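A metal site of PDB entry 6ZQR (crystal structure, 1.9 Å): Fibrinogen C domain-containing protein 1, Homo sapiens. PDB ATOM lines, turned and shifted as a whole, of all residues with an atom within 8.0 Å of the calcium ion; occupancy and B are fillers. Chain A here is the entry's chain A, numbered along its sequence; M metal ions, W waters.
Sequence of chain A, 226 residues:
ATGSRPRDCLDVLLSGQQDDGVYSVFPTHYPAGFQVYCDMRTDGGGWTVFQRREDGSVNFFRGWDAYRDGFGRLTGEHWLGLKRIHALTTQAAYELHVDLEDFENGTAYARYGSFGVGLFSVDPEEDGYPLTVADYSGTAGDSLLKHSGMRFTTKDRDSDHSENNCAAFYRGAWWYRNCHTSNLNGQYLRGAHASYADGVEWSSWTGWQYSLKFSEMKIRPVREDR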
ATOM      1  N   THR A 153      24.272  15.581   0.594  1.00  0.00           N
ATOM      2  CA  THR A 153      23.746  14.994   1.861  1.00  0.00           C
ATOM      3  C   THR A 153      22.233  14.842   1.785  1.00  0.00           C
ATOM      4  O   THR A 153      21.527  15.817   1.442  1.00  0.00           O
ATOM      5  CB  THR A 153      24.223  15.819   3.061  1.00  0.00           C
ATOM      6  OG1 THR A 153      25.603  15.519   3.241  1.00  0.00           O
ATOM      7  CG2 THR A 153      23.439  15.544   4.329  1.00  0.00           C
ATOM      8  N   ARG A 157      21.922   9.806   4.486  1.00  0.00           N
ATOM      9  CA  ARG A 157      23.364   9.752   4.134  1.00  0.00           C
ATOM     10  C   ARG A 157      24.040  11.103   4.403  1.00  0.00           C
ATOM     11  O   ARG A 157      23.962  12.008   3.531  1.00  0.00           O
ATOM     12  CB  ARG A 157      23.555   9.292   2.690  1.00  0.00           C
ATOM     13  CG  ARG A 157      24.938   8.705   2.413  1.00  0.00           C
ATOM     14  CD  ARG A 157      25.088   8.341   0.945  1.00  0.00           C
ATOM     15  NE  ARG A 157      26.344   7.646   0.651  1.00  0.00           N
ATOM     16  CZ  ARG A 157      27.508   8.242   0.373  1.00  0.00           C
ATOM     17  NH1 ARG A 157      27.612   9.555   0.353  1.00  0.00           N
ATOM     18  NH2 ARG A 157      28.574   7.502   0.119  1.00  0.00           N
ATOM     19  N   ASP A 158      24.710  11.218   5.547  1.00  0.00           N
ATOM     20  CA  ASP A 158      25.331  12.449   6.078  1.00  0.00           C
ATOM     21  C   ASP A 158      26.796  12.561   5.630  1.00  0.00           C
ATOM     22  O   ASP A 158      27.610  11.756   6.100  1.00  0.00           O
ATOM     23  CB  ASP A 158      25.234  12.459   7.615  1.00  0.00           C
ATOM     24  CG  ASP A 158      25.693  13.750   8.244  1.00  0.00           C
ATOM     25  OD1 ASP A 158      26.465  14.496   7.591  1.00  0.00           O
ATOM     26  OD2 ASP A 158      25.244  14.037   9.357  1.00  0.00           O
ATOM     27  N   SER A 159      27.117  13.552   4.787  1.00  0.00           N
ATOM     28  CA  SER A 159      28.511  13.900   4.381  1.00  0.00           C
ATOM     29  C   SER A 159      28.773  15.394   4.567  1.00  0.00           C
ATOM     30  O   SER A 159      29.654  15.926   3.855  1.00  0.00           O
ATOM     31  CB  SER A 159      28.819  13.491   2.967  1.00  0.00           C
ATOM     32  OG  SER A 159      28.444  12.140   2.734  1.00  0.00           O
ATOM     33  N   ASP A 160      28.067  16.051   5.496  1.00  0.00           N
ATOM     34  CA  ASP A 160      28.084  17.528   5.654  1.00  0.00           C
ATOM     35  C   ASP A 160      29.145  17.917   6.699  1.00  0.00           C
ATOM     36  O   ASP A 160      29.831  17.006   7.215  1.00  0.00           O
ATOM     37  CB  ASP A 160      26.681  18.049   5.981  1.00  0.00           C
ATOM     38  CG  ASP A 160      26.124  17.584   7.307  1.00  0.00           C
ATOM     39  OD1 ASP A 160      26.930  17.440   8.257  1.00  0.00           O
ATOM     40  OD2 ASP A 160      24.900  17.370   7.396  1.00  0.00           O
ATOM     41  N   HIS A 161      29.284  19.212   6.991  1.00  0.00           N
ATOM     42  CA  HIS A 161      30.267  19.755   7.977  1.00  0.00           C
ATOM     43  C   HIS A 161      29.562  20.134   9.283  1.00  0.00           C
ATOM     44  O   HIS A 161      30.136  20.934  10.029  1.00  0.00           O
ATOM     45  CB  HIS A 161      31.019  20.957   7.389  1.00  0.00           C
ATOM     46  CG  HIS A 161      32.087  20.573   6.409  1.00  0.00           C
ATOM     47  ND1 HIS A 161      32.228  19.284   5.936  1.00  0.00           N
ATOM     48  CD2 HIS A 161      33.035  21.316   5.805  1.00  0.00           C
ATOM     49  CE1 HIS A 161      33.237  19.244   5.086  1.00  0.00           C
ATOM     50  NE2 HIS A 161      33.744  20.477   4.984  1.00  0.00           N
ATOM     51  N   SER A 162      28.378  19.580   9.537  1.00  0.00           N
ATOM     52  CA  SER A 162      27.611  19.780  10.798  1.00  0.00           C
ATOM     53  C   SER A 162      27.818  18.565  11.705  1.00  0.00           C
ATOM     54  O   SER A 162      28.027  17.443  11.179  1.00  0.00           O
ATOM     55  CB  SER A 162      26.154  20.011  10.527  1.00  0.00           C
ATOM     56  OG  SER A 162      25.408  19.979  11.746  1.00  0.00           O
ATOM     57  N   GLU A 163      27.711  18.772  13.020  1.00  0.00           N
ATOM     58  CA  GLU A 163      27.613  17.685  14.024  1.00  0.00           C
ATOM     59  C   GLU A 163      26.229  17.030  13.862  1.00  0.00           C
ATOM     60  O   GLU A 163      26.095  15.868  14.249  1.00  0.00           O
ATOM     61  CB  GLU A 163      27.854  18.227  15.429  1.00  0.00           C
ATOM     62  CG  GLU A 163      29.213  18.909  15.582  1.00  0.00           C
ATOM     63  CD  GLU A 163      29.400  19.654  16.897  1.00  0.00           C
ATOM     64  OE1 GLU A 163      29.473  18.985  17.954  1.00  0.00           O
ATOM     65  OE2 GLU A 163      29.463  20.900  16.870  1.00  0.00           O
ATOM     66  N   ASN A 164      25.268  17.742  13.268  1.00  0.00           N
ATOM     67  CA  ASN A 164      23.916  17.208  12.915  1.00  0.00           C
ATOM     68  C   ASN A 164      23.891  16.770  11.438  1.00  0.00           C
ATOM     69  O   ASN A 164      24.908  16.946  10.738  1.00  0.00           O
ATOM     70  CB  ASN A 164      22.832  18.268  13.161  1.00  0.00           C
ATOM     71  CG  ASN A 164      22.832  18.754  14.593  1.00  0.00           C
ATOM     72  OD1 ASN A 164      22.916  17.954  15.529  1.00  0.00           O
ATOM     73  ND2 ASN A 164      22.745  20.056  14.772  1.00  0.00           N
ATOM     74  N   ASN A 165      22.762  16.185  11.003  1.00  0.00           N
ATOM     75  CA  ASN A 165      22.433  15.955   9.572  1.00  0.00           C
ATOM     76  C   ASN A 165      21.651  17.178   9.071  1.00  0.00           C
ATOM     77  O   ASN A 165      20.476  17.312   9.443  1.00  0.00           O
ATOM     78  CB  ASN A 165      21.663  14.638   9.398  1.00  0.00           C
ATOM     79  CG  ASN A 165      21.406  14.322   7.948  1.00  0.00           C
ATOM     80  OD1 ASN A 165      21.103  15.222   7.173  1.00  0.00           O
ATOM     81  ND2 ASN A 165      21.549  13.063   7.549  1.00  0.00           N
ATOM     82  N   CYS A 166      22.301  18.041   8.287  1.00  0.00           N
ATOM     83  CA  CYS A 166      21.737  19.284   7.681  1.00  0.00           C
ATOM     84  C   CYS A 166      20.456  18.963   6.894  1.00  0.00           C
ATOM     85  O   CYS A 166      19.492  19.789   6.940  1.00  0.00           O
ATOM     86  CB  CYS A 166      22.757  19.973   6.790  1.00  0.00           C
ATOM     87  SG  CYS A 166      24.183  20.659   7.673  1.00  0.00           S
ATOM     88  N   ALA A 167      20.394  17.798   6.231  1.00  0.00           N
ATOM     89  CA  ALA A 167      19.255  17.389   5.376  1.00  0.00           C
ATOM     90  C   ALA A 167      18.028  17.135   6.262  1.00  0.00           C
ATOM     91  O   ALA A 167      16.945  17.639   5.931  1.00  0.00           O
ATOM     92  CB  ALA A 167      19.613  16.175   4.559  1.00  0.00           C
ATOM     93  N   TYR A 176      25.328  20.302   1.410  1.00  0.00           N
ATOM     94  CA  TYR A 176      25.305  21.049   2.689  1.00  0.00           C
ATOM     95  C   TYR A 176      26.731  21.202   3.257  1.00  0.00           C
ATOM     96  O   TYR A 176      27.558  20.254   3.177  1.00  0.00           O
ATOM     97  CB  TYR A 176      24.413  20.347   3.712  1.00  0.00           C
ATOM     98  CG  TYR A 176      22.933  20.434   3.436  1.00  0.00           C
ATOM     99  CD1 TYR A 176      22.246  21.642   3.549  1.00  0.00           C
ATOM    100  CD2 TYR A 176      22.210  19.306   3.115  1.00  0.00           C
ATOM    101  CE1 TYR A 176      20.877  21.711   3.326  1.00  0.00           C
ATOM    102  CE2 TYR A 176      20.843  19.346   2.915  1.00  0.00           C
ATOM    103  CZ  TYR A 176      20.179  20.556   3.013  1.00  0.00           C
ATOM    104  OH  TYR A 176      18.840  20.582   2.815  1.00  0.00           O
ATOM    105  N   ARG A 177      27.008  22.385   3.824  1.00  0.00           N
ATOM    106  CA  ARG A 177      28.249  22.639   4.604  1.00  0.00           C
ATOM    107  C   ARG A 177      27.858  22.613   6.085  1.00  0.00           C
ATOM    108  O   ARG A 177      27.810  21.513   6.681  1.00  0.00           O
ATOM    109  CB  ARG A 177      28.913  23.937   4.141  1.00  0.00           C
ATOM    110  CG  ARG A 177      30.235  24.237   4.845  1.00  0.00           C
ATOM    111  CD  ARG A 177      30.894  25.536   4.414  1.00  0.00           C
ATOM    112  NE  ARG A 177      31.187  25.470   2.989  1.00  0.00           N
ATOM    113  CZ  ARG A 177      32.228  24.833   2.451  1.00  0.00           C
ATOM    114  NH1 ARG A 177      33.137  24.241   3.218  1.00  0.00           N
ATOM    115  NH2 ARG A 177      32.375  24.812   1.135  1.00  0.00           N
ATOM    116  N   ASN A 178      27.529  23.780   6.640  1.00  0.00           N
ATOM    117  CA  ASN A 178      27.136  23.930   8.066  1.00  0.00           C
ATOM    118  C   ASN A 178      26.276  25.189   8.208  1.00  0.00           C
ATOM    119  O   ASN A 178      26.697  26.141   8.858  1.00  0.00           O
ATOM    120  CB  ASN A 178      28.387  23.991   8.951  1.00  0.00           C
ATOM    121  CG  ASN A 178      28.061  23.765  10.411  1.00  0.00           C
ATOM    122  OD1 ASN A 178      27.090  23.090  10.741  1.00  0.00           O
ATOM    123  ND2 ASN A 178      28.879  24.308  11.286  1.00  0.00           N
ATOM    124  N   CYS A 179      25.088  25.214   7.565  1.00  0.00           N
ATOM    125  CA  CYS A 179      24.544  24.139   6.745  1.00  0.00           C
ATOM    126  C   CYS A 179      24.355  24.627   5.300  1.00  0.00           C
ATOM    127  O   CYS A 179      24.809  23.896   4.389  1.00  0.00           O
ATOM    128  CB  CYS A 179      23.230  23.620   7.300  1.00  0.00           C
ATOM    129  SG  CYS A 179      23.454  22.397   8.624  1.00  0.00           S
HETATM  130 CA    CA M   1      26.711  15.768   9.755  1.00  0.00          CA
HETATM  131  O   HOH W   1      27.265  14.285  11.823  1.00  0.00           O
HETATM  132  O   HOH W   2      29.064  15.301   9.103  1.00  0.00           O
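Of the 16 residues printed, 4 come within 4 Å of the calcium ion.
The backbone NH (N) of Asp 160 is in hydrogen-bond range of the side-chain hydroxyl (OG1) of Thr 153, 3.4 Å away.
The side-chain sulfur (SG) of Cys 179 is disulfide-bonded to the side-chain sulfur (SG) of Cys 166 (2.1 Å).
The side-chain carboxylate of Asp 160 sits at hydrogen-bond distance from the backbone NH of Cys 166.
The backbone NH (N) of Ser 162 is in hydrogen-bond range of the backbone carbonyl oxygen (O) of Arg 177, at 3.5 Å.
N of Asn 164 sits at hydrogen-bond distance from OG of Ser 162, at 2.7 Å.
The calcium ion is bound by OD1 of Asp 160.
The calcium ion is bound by OD2 of Asp 158, 2.3 Å away.
The calcium ion is bound by O of Asn 164 (2.4 Å).
Water W2 binds the calcium ion, 2.5 Å away.
OD1 of Asp 158 binds the calcium ion.
O of Ser 162 binds the calcium ion (2.6 Å).
Water W1 is bound to the calcium ion, at 2.6 Å.
The calcium ion has seven donor atoms within binding distance.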
